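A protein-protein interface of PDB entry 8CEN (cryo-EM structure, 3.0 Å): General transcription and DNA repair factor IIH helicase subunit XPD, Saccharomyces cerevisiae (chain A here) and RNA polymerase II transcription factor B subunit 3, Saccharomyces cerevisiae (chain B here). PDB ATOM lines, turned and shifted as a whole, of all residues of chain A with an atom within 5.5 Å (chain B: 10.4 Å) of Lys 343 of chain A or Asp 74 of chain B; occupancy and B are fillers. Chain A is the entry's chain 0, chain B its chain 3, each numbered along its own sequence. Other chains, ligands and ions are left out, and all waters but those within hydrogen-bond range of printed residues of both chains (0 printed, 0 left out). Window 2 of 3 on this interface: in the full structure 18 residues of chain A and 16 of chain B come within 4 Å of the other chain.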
ATOM      1  N   LEU A 257       3.773  -6.318  -7.878  1.00  0.00           N
ATOM      2  CA  LEU A 257       3.500  -5.010  -7.286  1.00  0.00           C
ATOM      3  C   LEU A 257       3.186  -5.103  -5.795  1.00  0.00           C
ATOM      4  O   LEU A 257       3.526  -4.187  -5.039  1.00  0.00           O
ATOM      5  CB  LEU A 257       2.359  -4.317  -8.025  1.00  0.00           C
ATOM      6  CG  LEU A 257       2.723  -3.790  -9.412  1.00  0.00           C
ATOM      7  CD1 LEU A 257       1.612  -2.937  -9.947  1.00  0.00           C
ATOM      8  CD2 LEU A 257       3.994  -2.984  -9.347  1.00  0.00           C
ATOM      9  N   THR A 261       5.303  -3.146  -3.012  1.00  0.00           N
ATOM     10  CA  THR A 261       4.806  -2.321  -1.912  1.00  0.00           C
ATOM     11  C   THR A 261       5.388  -2.775  -0.579  1.00  0.00           C
ATOM     12  O   THR A 261       5.796  -1.944   0.245  1.00  0.00           O
ATOM     13  CB  THR A 261       3.279  -2.360  -1.859  1.00  0.00           C
ATOM     14  OG1 THR A 261       2.832  -3.721  -1.845  1.00  0.00           O
ATOM     15  CG2 THR A 261       2.676  -1.640  -3.053  1.00  0.00           C
ATOM     16  N   LEU A 338       5.377   5.714  -7.533  1.00  0.00           N
ATOM     17  CA  LEU A 338       5.484   5.053  -8.833  1.00  0.00           C
ATOM     18  C   LEU A 338       4.821   3.677  -8.819  1.00  0.00           C
ATOM     19  O   LEU A 338       4.103   3.312  -9.761  1.00  0.00           O
ATOM     20  CB  LEU A 338       6.954   4.933  -9.237  1.00  0.00           C
ATOM     21  CG  LEU A 338       7.256   4.107 -10.489  1.00  0.00           C
ATOM     22  CD1 LEU A 338       6.737   4.808 -11.734  1.00  0.00           C
ATOM     23  CD2 LEU A 338       8.746   3.828 -10.603  1.00  0.00           C
ATOM     24  N   ILE A 339       5.043   2.905  -7.751  1.00  0.00           N
ATOM     25  CA  ILE A 339       4.432   1.583  -7.634  1.00  0.00           C
ATOM     26  C   ILE A 339       2.916   1.701  -7.513  1.00  0.00           C
ATOM     27  O   ILE A 339       2.168   0.906  -8.100  1.00  0.00           O
ATOM     28  CB  ILE A 339       5.054   0.822  -6.447  1.00  0.00           C
ATOM     29  CG1 ILE A 339       6.514   0.485  -6.742  1.00  0.00           C
ATOM     30  CG2 ILE A 339       4.300  -0.461  -6.154  1.00  0.00           C
ATOM     31  CD1 ILE A 339       7.312   0.108  -5.516  1.00  0.00           C
ATOM     32  N   GLU A 340       2.435   2.708  -6.780  1.00  0.00           N
ATOM     33  CA  GLU A 340       0.993   2.923  -6.682  1.00  0.00           C
ATOM     34  C   GLU A 340       0.396   3.338  -8.023  1.00  0.00           C
ATOM     35  O   GLU A 340      -0.722   2.931  -8.360  1.00  0.00           O
ATOM     36  CB  GLU A 340       0.689   3.960  -5.605  1.00  0.00           C
ATOM     37  CG  GLU A 340       0.779   3.400  -4.199  1.00  0.00           C
ATOM     38  CD  GLU A 340      -0.073   2.162  -4.015  1.00  0.00           C
ATOM     39  OE1 GLU A 340      -1.280   2.215  -4.329  1.00  0.00           O
ATOM     40  OE2 GLU A 340       0.466   1.132  -3.560  1.00  0.00           O
ATOM     41  N   TYR A 341       1.130   4.137  -8.808  1.00  0.00           N
ATOM     42  CA  TYR A 341       0.676   4.468 -10.155  1.00  0.00           C
ATOM     43  C   TYR A 341       0.591   3.224 -11.031  1.00  0.00           C
ATOM     44  O   TYR A 341      -0.335   3.087 -11.838  1.00  0.00           O
ATOM     45  CB  TYR A 341       1.604   5.503 -10.787  1.00  0.00           C
ATOM     46  CG  TYR A 341       1.278   5.805 -12.233  1.00  0.00           C
ATOM     47  CD1 TYR A 341       0.231   6.653 -12.562  1.00  0.00           C
ATOM     48  CD2 TYR A 341       2.017   5.243 -13.267  1.00  0.00           C
ATOM     49  CE1 TYR A 341      -0.073   6.934 -13.878  1.00  0.00           C
ATOM     50  CE2 TYR A 341       1.720   5.520 -14.585  1.00  0.00           C
ATOM     51  CZ  TYR A 341       0.674   6.363 -14.884  1.00  0.00           C
ATOM     52  OH  TYR A 341       0.375   6.640 -16.197  1.00  0.00           O
ATOM     53  N   LEU A 342       1.560   2.315 -10.893  1.00  0.00           N
ATOM     54  CA  LEU A 342       1.508   1.055 -11.634  1.00  0.00           C
ATOM     55  C   LEU A 342       0.306   0.212 -11.214  1.00  0.00           C
ATOM     56  O   LEU A 342      -0.338  -0.436 -12.054  1.00  0.00           O
ATOM     57  CB  LEU A 342       2.809   0.280 -11.432  1.00  0.00           C
ATOM     58  CG  LEU A 342       4.052   0.868 -12.102  1.00  0.00           C
ATOM     59  CD1 LEU A 342       5.251  -0.039 -11.895  1.00  0.00           C
ATOM     60  CD2 LEU A 342       3.805   1.107 -13.582  1.00  0.00           C
ATOM     61  N   LYS A 343      -0.007   0.211  -9.913  1.00  0.00           N
ATOM     62  CA  LYS A 343      -1.184  -0.505  -9.425  1.00  0.00           C
ATOM     63  C   LYS A 343      -2.469   0.083  -9.995  1.00  0.00           C
ATOM     64  O   LYS A 343      -3.403  -0.655 -10.327  1.00  0.00           O
ATOM     65  CB  LYS A 343      -1.225  -0.489  -7.896  1.00  0.00           C
ATOM     66  CG  LYS A 343      -0.108  -1.271  -7.228  1.00  0.00           C
ATOM     67  CD  LYS A 343      -0.223  -1.257  -5.716  1.00  0.00           C
ATOM     68  CE  LYS A 343      -1.375  -2.123  -5.241  1.00  0.00           C
ATOM     69  NZ  LYS A 343      -1.419  -2.213  -3.756  1.00  0.00           N
ATOM     70  N   THR A 344      -2.538   1.412 -10.108  1.00  0.00           N
ATOM     71  CA  THR A 344      -3.700   2.038 -10.736  1.00  0.00           C
ATOM     72  C   THR A 344      -3.775   1.715 -12.223  1.00  0.00           C
ATOM     73  O   THR A 344      -4.870   1.531 -12.768  1.00  0.00           O
ATOM     74  CB  THR A 344      -3.681   3.553 -10.532  1.00  0.00           C
ATOM     75  OG1 THR A 344      -2.510   4.108 -11.140  1.00  0.00           O
ATOM     76  CG2 THR A 344      -3.709   3.893  -9.058  1.00  0.00           C
ATOM     77  N   ARG A 345      -2.623   1.658 -12.899  1.00  0.00           N
ATOM     78  CA  ARG A 345      -2.616   1.372 -14.331  1.00  0.00           C
ATOM     79  C   ARG A 345      -3.039  -0.059 -14.633  1.00  0.00           C
ATOM     80  O   ARG A 345      -3.657  -0.309 -15.674  1.00  0.00           O
ATOM     81  CB  ARG A 345      -1.235   1.643 -14.925  1.00  0.00           C
ATOM     82  CG  ARG A 345      -0.899   3.115 -15.086  1.00  0.00           C
ATOM     83  CD  ARG A 345      -2.020   3.870 -15.780  1.00  0.00           C
ATOM     84  NE  ARG A 345      -2.279   3.355 -17.119  1.00  0.00           N
ATOM     85  CZ  ARG A 345      -1.742   3.843 -18.228  1.00  0.00           C
ATOM     86  NH1 ARG A 345      -0.899   4.863 -18.197  1.00  0.00           N
ATOM     87  NH2 ARG A 345      -2.058   3.296 -19.398  1.00  0.00           N
ATOM     88  N   MET A 346      -2.718  -1.009 -13.754  1.00  0.00           N
ATOM     89  CA  MET A 346      -3.134  -2.383 -14.024  1.00  0.00           C
ATOM     90  C   MET A 346      -4.610  -2.648 -13.741  1.00  0.00           C
ATOM     91  O   MET A 346      -5.098  -3.726 -14.096  1.00  0.00           O
ATOM     92  CB  MET A 346      -2.278  -3.383 -13.246  1.00  0.00           C
ATOM     93  CG  MET A 346      -0.838  -3.421 -13.710  1.00  0.00           C
ATOM     94  SD  MET A 346       0.190  -4.540 -12.751  1.00  0.00           S
ATOM     95  CE  MET A 346      -0.443  -6.121 -13.278  1.00  0.00           C
ATOM     96  N   LYS A 347      -5.333  -1.718 -13.118  1.00  0.00           N
ATOM     97  CA  LYS A 347      -6.775  -1.887 -12.918  1.00  0.00           C
ATOM     98  C   LYS A 347      -7.537  -1.284 -14.100  1.00  0.00           C
ATOM     99  O   LYS A 347      -8.272  -0.300 -13.987  1.00  0.00           O
ATOM    100  CB  LYS A 347      -7.210  -1.279 -11.590  1.00  0.00           C
ATOM    101  CG  LYS A 347      -6.626  -1.984 -10.371  1.00  0.00           C
ATOM    102  CD  LYS A 347      -6.449  -1.041  -9.190  1.00  0.00           C
ATOM    103  CE  LYS A 347      -7.739  -0.318  -8.847  1.00  0.00           C
ATOM    104  NZ  LYS A 347      -7.538   0.665  -7.747  1.00  0.00           N
ATOM    105  N   ASN B   9     -11.855  -0.725   7.006  1.00  0.00           N
ATOM    106  CA  ASN B   9     -11.712  -1.774   6.004  1.00  0.00           C
ATOM    107  C   ASN B   9     -11.654  -1.177   4.600  1.00  0.00           C
ATOM    108  O   ASN B   9     -12.280  -0.154   4.324  1.00  0.00           O
ATOM    109  CB  ASN B   9     -12.865  -2.776   6.108  1.00  0.00           C
ATOM    110  CG  ASN B   9     -12.622  -4.033   5.294  1.00  0.00           C
ATOM    111  OD1 ASN B   9     -11.494  -4.318   4.891  1.00  0.00           O
ATOM    112  ND2 ASN B   9     -13.683  -4.794   5.051  1.00  0.00           N
ATOM    113  N   LYS B  10     -10.897  -1.826   3.716  1.00  0.00           N
ATOM    114  CA  LYS B  10     -10.736  -1.357   2.346  1.00  0.00           C
ATOM    115  C   LYS B  10     -11.903  -1.737   1.444  1.00  0.00           C
ATOM    116  O   LYS B  10     -11.945  -1.288   0.293  1.00  0.00           O
ATOM    117  CB  LYS B  10      -9.436  -1.904   1.745  1.00  0.00           C
ATOM    118  CG  LYS B  10      -8.182  -1.098   2.074  1.00  0.00           C
ATOM    119  CD  LYS B  10      -7.625  -1.434   3.452  1.00  0.00           C
ATOM    120  CE  LYS B  10      -7.342  -2.923   3.587  1.00  0.00           C
ATOM    121  NZ  LYS B  10      -6.900  -3.284   4.963  1.00  0.00           N
ATOM    122  N   ASP B  11     -12.843  -2.545   1.931  1.00  0.00           N
ATOM    123  CA  ASP B  11     -13.955  -3.028   1.123  1.00  0.00           C
ATOM    124  C   ASP B  11     -15.289  -2.388   1.474  1.00  0.00           C
ATOM    125  O   ASP B  11     -16.157  -2.282   0.605  1.00  0.00           O
ATOM    126  CB  ASP B  11     -14.080  -4.553   1.262  1.00  0.00           C
ATOM    127  CG  ASP B  11     -15.127  -5.146   0.338  1.00  0.00           C
ATOM    128  OD1 ASP B  11     -14.865  -5.234  -0.881  1.00  0.00           O
ATOM    129  OD2 ASP B  11     -16.211  -5.522   0.830  1.00  0.00           O
ATOM    130  N   PHE B  28     -15.375   5.166  -3.449  1.00  0.00           N
ATOM    131  CA  PHE B  28     -14.133   5.425  -2.720  1.00  0.00           C
ATOM    132  C   PHE B  28     -13.903   6.928  -2.534  1.00  0.00           C
ATOM    133  O   PHE B  28     -12.888   7.485  -2.949  1.00  0.00           O
ATOM    134  CB  PHE B  28     -12.956   4.782  -3.448  1.00  0.00           C
ATOM    135  CG  PHE B  28     -12.902   3.281  -3.330  1.00  0.00           C
ATOM    136  CD1 PHE B  28     -13.681   2.608  -2.403  1.00  0.00           C
ATOM    137  CD2 PHE B  28     -12.067   2.546  -4.157  1.00  0.00           C
ATOM    138  CE1 PHE B  28     -13.626   1.228  -2.301  1.00  0.00           C
ATOM    139  CE2 PHE B  28     -12.007   1.167  -4.060  1.00  0.00           C
ATOM    140  CZ  PHE B  28     -12.789   0.508  -3.130  1.00  0.00           C
ATOM    141  N   VAL B  30     -12.947  10.248  -0.601  1.00  0.00           N
ATOM    142  CA  VAL B  30     -12.082  10.718   0.472  1.00  0.00           C
ATOM    143  C   VAL B  30     -12.059  12.241   0.441  1.00  0.00           C
ATOM    144  O   VAL B  30     -12.558  12.876  -0.488  1.00  0.00           O
ATOM    145  CB  VAL B  30     -10.644  10.161   0.371  1.00  0.00           C
ATOM    146  CG1 VAL B  30     -10.628   8.648   0.537  1.00  0.00           C
ATOM    147  CG2 VAL B  30     -10.012  10.566  -0.952  1.00  0.00           C
ATOM    148  N   TYR B  35      -8.390  11.928   5.129  1.00  0.00           N
ATOM    149  CA  TYR B  35      -8.672  10.860   4.176  1.00  0.00           C
ATOM    150  C   TYR B  35      -9.387   9.728   4.902  1.00  0.00           C
ATOM    151  O   TYR B  35      -8.783   9.018   5.713  1.00  0.00           O
ATOM    152  CB  TYR B  35      -7.384  10.376   3.517  1.00  0.00           C
ATOM    153  CG  TYR B  35      -6.796  11.395   2.576  1.00  0.00           C
ATOM    154  CD1 TYR B  35      -5.981  12.412   3.052  1.00  0.00           C
ATOM    155  CD2 TYR B  35      -7.078  11.363   1.217  1.00  0.00           C
ATOM    156  CE1 TYR B  35      -5.454  13.355   2.208  1.00  0.00           C
ATOM    157  CE2 TYR B  35      -6.552  12.307   0.360  1.00  0.00           C
ATOM    158  CZ  TYR B  35      -5.739  13.299   0.865  1.00  0.00           C
ATOM    159  OH  TYR B  35      -5.207  14.249   0.031  1.00  0.00           O
ATOM    160  N   HIS B  36     -10.672   9.560   4.607  1.00  0.00           N
ATOM    161  CA  HIS B  36     -11.507   8.564   5.256  1.00  0.00           C
ATOM    162  C   HIS B  36     -12.195   7.725   4.193  1.00  0.00           C
ATOM    163  O   HIS B  36     -12.677   8.259   3.189  1.00  0.00           O
ATOM    164  CB  HIS B  36     -12.560   9.223   6.150  1.00  0.00           C
ATOM    165  CG  HIS B  36     -11.990   9.914   7.348  1.00  0.00           C
ATOM    166  ND1 HIS B  36     -11.296   9.250   8.337  1.00  0.00           N
ATOM    167  CD2 HIS B  36     -12.001  11.219   7.707  1.00  0.00           C
ATOM    168  CE1 HIS B  36     -10.912  10.116   9.259  1.00  0.00           C
ATOM    169  NE2 HIS B  36     -11.328  11.318   8.901  1.00  0.00           N
ATOM    170  N   ARG B  37     -12.239   6.413   4.412  1.00  0.00           N
ATOM    171  CA  ARG B  37     -12.999   5.548   3.521  1.00  0.00           C
ATOM    172  C   ARG B  37     -14.478   5.789   3.797  1.00  0.00           C
ATOM    173  O   ARG B  37     -15.055   5.201   4.717  1.00  0.00           O
ATOM    174  CB  ARG B  37     -12.608   4.079   3.724  1.00  0.00           C
ATOM    175  CG  ARG B  37     -13.453   3.052   2.968  1.00  0.00           C
ATOM    176  CD  ARG B  37     -13.462   3.309   1.469  1.00  0.00           C
ATOM    177  NE  ARG B  37     -14.497   2.539   0.789  1.00  0.00           N
ATOM    178  CZ  ARG B  37     -15.672   3.025   0.414  1.00  0.00           C
ATOM    179  NH1 ARG B  37     -15.998   4.289   0.626  1.00  0.00           N
ATOM    180  NH2 ARG B  37     -16.542   2.224  -0.195  1.00  0.00           N
ATOM    181  N   LYS B  69     -13.622  13.871  -3.164  1.00  0.00           N
ATOM    182  CA  LYS B  69     -13.193  13.328  -4.445  1.00  0.00           C
ATOM    183  C   LYS B  69     -12.894  11.851  -4.246  1.00  0.00           C
ATOM    184  O   LYS B  69     -12.765  11.370  -3.118  1.00  0.00           O
ATOM    185  CB  LYS B  69     -11.966  14.067  -4.988  1.00  0.00           C
ATOM    186  CG  LYS B  69     -10.706  13.840  -4.168  1.00  0.00           C
ATOM    187  CD  LYS B  69      -9.524  14.606  -4.734  1.00  0.00           C
ATOM    188  CE  LYS B  69      -8.282  14.401  -3.882  1.00  0.00           C
ATOM    189  NZ  LYS B  69      -7.799  12.993  -3.938  1.00  0.00           N
ATOM    190  N   THR B  70     -12.785  11.132  -5.359  1.00  0.00           N
ATOM    191  CA  THR B  70     -12.419   9.726  -5.298  1.00  0.00           C
ATOM    192  C   THR B  70     -10.905   9.580  -5.196  1.00  0.00           C
ATOM    193  O   THR B  70     -10.147  10.405  -5.716  1.00  0.00           O
ATOM    194  CB  THR B  70     -12.966   8.969  -6.515  1.00  0.00           C
ATOM    195  OG1 THR B  70     -12.714   7.565  -6.363  1.00  0.00           O
ATOM    196  CG2 THR B  70     -12.355   9.470  -7.821  1.00  0.00           C
ATOM    197  N   GLN B  71     -10.467   8.554  -4.473  1.00  0.00           N
ATOM    198  CA  GLN B  71      -9.042   8.310  -4.313  1.00  0.00           C
ATOM    199  C   GLN B  71      -8.505   7.541  -5.512  1.00  0.00           C
ATOM    200  O   GLN B  71      -9.100   6.555  -5.955  1.00  0.00           O
ATOM    201  CB  GLN B  71      -8.759   7.538  -3.024  1.00  0.00           C
ATOM    202  CG  GLN B  71      -9.722   6.401  -2.742  1.00  0.00           C
ATOM    203  CD  GLN B  71      -9.478   5.753  -1.393  1.00  0.00           C
ATOM    204  OE1 GLN B  71      -8.334   5.527  -0.999  1.00  0.00           O
ATOM    205  NE2 GLN B  71     -10.555   5.445  -0.680  1.00  0.00           N
ATOM    206  N   ILE B  72      -7.375   8.005  -6.041  1.00  0.00           N
ATOM    207  CA  ILE B  72      -6.767   7.331  -7.180  1.00  0.00           C
ATOM    208  C   ILE B  72      -5.959   6.127  -6.719  1.00  0.00           C
ATOM    209  O   ILE B  72      -6.132   5.014  -7.227  1.00  0.00           O
ATOM    210  CB  ILE B  72      -5.900   8.318  -7.985  1.00  0.00           C
ATOM    211  CG1 ILE B  72      -6.657   9.627  -8.218  1.00  0.00           C
ATOM    212  CG2 ILE B  72      -5.481   7.703  -9.309  1.00  0.00           C
ATOM    213  CD1 ILE B  72      -5.797  10.737  -8.781  1.00  0.00           C
ATOM    214  N   PHE B  73      -5.097   6.321  -5.729  1.00  0.00           N
ATOM    215  CA  PHE B  73      -4.168   5.292  -5.293  1.00  0.00           C
ATOM    216  C   PHE B  73      -4.757   4.466  -4.155  1.00  0.00           C
ATOM    217  O   PHE B  73      -5.704   4.873  -3.478  1.00  0.00           O
ATOM    218  CB  PHE B  73      -2.848   5.924  -4.856  1.00  0.00           C
ATOM    219  CG  PHE B  73      -2.256   6.846  -5.879  1.00  0.00           C
ATOM    220  CD1 PHE B  73      -1.886   6.372  -7.127  1.00  0.00           C
ATOM    221  CD2 PHE B  73      -2.086   8.190  -5.601  1.00  0.00           C
ATOM    222  CE1 PHE B  73      -1.345   7.221  -8.073  1.00  0.00           C
ATOM    223  CE2 PHE B  73      -1.551   9.044  -6.543  1.00  0.00           C
ATOM    224  CZ  PHE B  73      -1.177   8.559  -7.778  1.00  0.00           C
ATOM    225  N   ASP B  74      -4.179   3.280  -3.957  1.00  0.00           N
ATOM    226  CA  ASP B  74      -4.635   2.388  -2.898  1.00  0.00           C
ATOM    227  C   ASP B  74      -4.146   2.829  -1.524  1.00  0.00           C
ATOM    228  O   ASP B  74      -4.852   2.632  -0.529  1.00  0.00           O
ATOM    229  CB  ASP B  74      -4.176   0.957  -3.185  1.00  0.00           C
ATOM    230  CG  ASP B  74      -4.737  -0.046  -2.196  1.00  0.00           C
ATOM    231  OD1 ASP B  74      -5.941  -0.364  -2.288  1.00  0.00           O
ATOM    232  OD2 ASP B  74      -3.973  -0.517  -1.328  1.00  0.00           O
ATOM    233  N   ASP B  75      -2.957   3.421  -1.444  1.00  0.00           N
ATOM    234  CA  ASP B  75      -2.374   3.812  -0.168  1.00  0.00           C
ATOM    235  C   ASP B  75      -2.809   5.222   0.211  1.00  0.00           C
ATOM    236  O   ASP B  75      -2.732   6.148  -0.605  1.00  0.00           O
ATOM    237  CB  ASP B  75      -0.848   3.730  -0.215  1.00  0.00           C
ATOM    238  CG  ASP B  75      -0.342   2.305  -0.306  1.00  0.00           C
ATOM    239  OD1 ASP B  75      -1.031   1.394   0.197  1.00  0.00           O
ATOM    240  OD2 ASP B  75       0.754   2.100  -0.869  1.00  0.00           O
ATOM    241  N   VAL B  76      -3.261   5.371   1.459  1.00  0.00           N
ATOM    242  CA  VAL B  76      -3.679   6.672   1.974  1.00  0.00           C
ATOM    243  C   VAL B  76      -2.497   7.632   2.036  1.00  0.00           C
ATOM    244  O   VAL B  76      -2.614   8.811   1.674  1.00  0.00           O
ATOM    245  CB  VAL B  76      -4.344   6.497   3.353  1.00  0.00           C
ATOM    246  CG1 VAL B  76      -4.783   7.834   3.915  1.00  0.00           C
ATOM    247  CG2 VAL B  76      -5.523   5.540   3.252  1.00  0.00           C
ATOM    248  N   GLU B  77      -1.343   7.144   2.502  1.00  0.00           N
ATOM    249  CA  GLU B  77      -0.160   7.992   2.600  1.00  0.00           C
ATOM    250  C   GLU B  77       0.343   8.412   1.222  1.00  0.00           C
ATOM    251  O   GLU B  77       0.777   9.555   1.039  1.00  0.00           O
ATOM    252  CB  GLU B  77       0.930   7.285   3.417  1.00  0.00           C
ATOM    253  CG  GLU B  77       1.582   6.058   2.779  1.00  0.00           C
ATOM    254  CD  GLU B  77       0.801   4.772   3.005  1.00  0.00           C
ATOM    255  OE1 GLU B  77      -0.385   4.839   3.391  1.00  0.00           O
ATOM    256  OE2 GLU B  77       1.379   3.685   2.789  1.00  0.00           O
ATOM    257  N   VAL B  78       0.251   7.524   0.229  1.00  0.00           N
ATOM    258  CA  VAL B  78       0.642   7.891  -1.128  1.00  0.00           C
ATOM    259  C   VAL B  78      -0.332   8.912  -1.705  1.00  0.00           C
ATOM    260  O   VAL B  78       0.081   9.884  -2.349  1.00  0.00           O
ATOM    261  CB  VAL B  78       0.754   6.633  -2.009  1.00  0.00           C
ATOM    262  CG1 VAL B  78       0.928   7.008  -3.473  1.00  0.00           C
ATOM    263  CG2 VAL B  78       1.920   5.778  -1.543  1.00  0.00           C
ATOM    264  N   GLU B  79      -1.635   8.722  -1.463  1.00  0.00           N
ATOM    265  CA  GLU B  79      -2.639   9.666  -1.948  1.00  0.00           C
ATOM    266  C   GLU B  79      -2.425  11.057  -1.360  1.00  0.00           C
ATOM    267  O   GLU B  79      -2.434  12.062  -2.085  1.00  0.00           O
ATOM    268  CB  GLU B  79      -4.040   9.151  -1.611  1.00  0.00           C
ATOM    269  CG  GLU B  79      -5.185  10.031  -2.102  1.00  0.00           C
ATOM    270  CD  GLU B  79      -5.284  10.114  -3.614  1.00  0.00           C
ATOM    271  OE1 GLU B  79      -4.838   9.175  -4.304  1.00  0.00           O
ATOM    272  OE2 GLU B  79      -5.811  11.129  -4.116  1.00  0.00           O
ATOM    273  N   LYS B  80      -2.182  11.130  -0.048  1.00  0.00           N
ATOM    274  CA  LYS B  80      -1.955  12.431   0.573  1.00  0.00           C
ATOM    275  C   LYS B  80      -0.614  13.025   0.160  1.00  0.00           C
ATOM    276  O   LYS B  80      -0.498  14.250   0.044  1.00  0.00           O
ATOM    277  CB  LYS B  80      -2.074  12.330   2.099  1.00  0.00           C
ATOM    278  CG  LYS B  80      -0.945  11.622   2.822  1.00  0.00           C
ATOM    279  CD  LYS B  80      -1.251  11.470   4.302  1.00  0.00           C
ATOM    280  CE  LYS B  80      -1.296  12.821   4.997  1.00  0.00           C
ATOM    281  NZ  LYS B  80       0.037  13.483   5.017  1.00  0.00           N
ATOM    282  N   VAL B  82       0.868  12.666  -2.878  1.00  0.00           N
ATOM    283  CA  VAL B  82       0.695  13.251  -4.209  1.00  0.00           C
ATOM    284  C   VAL B  82      -0.223  14.472  -4.166  1.00  0.00           C
ATOM    285  O   VAL B  82      -0.023  15.424  -4.932  1.00  0.00           O
ATOM    286  CB  VAL B  82       0.211  12.196  -5.221  1.00  0.00           C
ATOM    287  CG1 VAL B  82       0.331  12.724  -6.638  1.00  0.00           C
ATOM    288  CG2 VAL B  82       1.087  10.970  -5.130  1.00  0.00           C
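OE1 of Glu 340 of chain A lies within hydrogen-bond range of N of Asp 74 of chain B.
NZ of Lys 343 of chain A lies within salt-bridge range of OD2 of Asp 74 of chain B.
OE2 of Glu 340 of chain A sits close to OD2 of Asp 75 of chain B, at 2.9 Å.
The side-chain amino group (NZ) of Lys 343 of chain A is in salt-bridge range of the side-chain carboxylate (OE2) of Glu 340 of chain A (3.8 Å).
O of Tyr 341 of chain A lies within hydrogen-bond range of OG1 of Thr 344 of chain A.
The side-chain hydroxyl (OH) of Tyr 341 of chain A lies within hydrogen-bond range of the guanidinium group (NH1) of Arg 345 of chain A (3.0 Å).
The backbone NH (N) of Ile 72 of chain B sits at hydrogen-bond distance from the side-chain carboxylate (OE1) of Glu 79 of chain B.
N of Phe 73 of chain B sits close to OE1 of Glu 79 of chain B (3.2 Å).
O of Glu 340 of chain A touches CD1 of Phe 73 of chain B, at 3.8 Å.
CG1 of Val 78 of chain B touches CG of Glu 340 of chain A, 3.7 Å away.
Phe 73 of chain B touches Tyr 341 of chain A.
Thr 344 of chain A touches Ile 72 of chain B.
CD1 of Phe 73 of chain B touches CG2 of Thr 344 of chain A (3.6 Å).
Of chain A, only Glu 340 and Lys 343 come within 4 Å of Asp 74 of chain B.
No residue of chain B comes within 4 Å of Leu 342 of chain A.
Thr 344 of chain A touches just these residues of chain B: Ile 72 (3.2 Å) and Phe 73 (3.6 Å).
No residue of chain B comes within 4 Å of Lys 347 of chain A.
Printed residues of chain A within 4 Å of Phe 73 of chain B: Glu 340, Tyr 341 and Thr 344.
Printed residues of chain A within 4 Å of Val 78 of chain B: Glu 340 (3.7 Å).
Of the printed residues of chain A, Ile 72 of chain B touches Thr 344.
Arg 345 of chain A touches none of the printed residues of chain B.
Leu 338 of chain A touches none of the printed residues of chain B.
The nearest residue of chain B that does not touch Lys 343 of chain A is Asp 75 of chain B (5.4 Å).
The nearest residue of chain A that does not touch Asp 74 of chain B is Thr 344 of chain A (5.2 Å).
The nearest printed residue of chain A that does not touch Asp 75 of chain B is Thr 261 of chain A (4.7 Å).
Of the 12 printed residues of chain A, 4 touch a printed residue of chain B.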
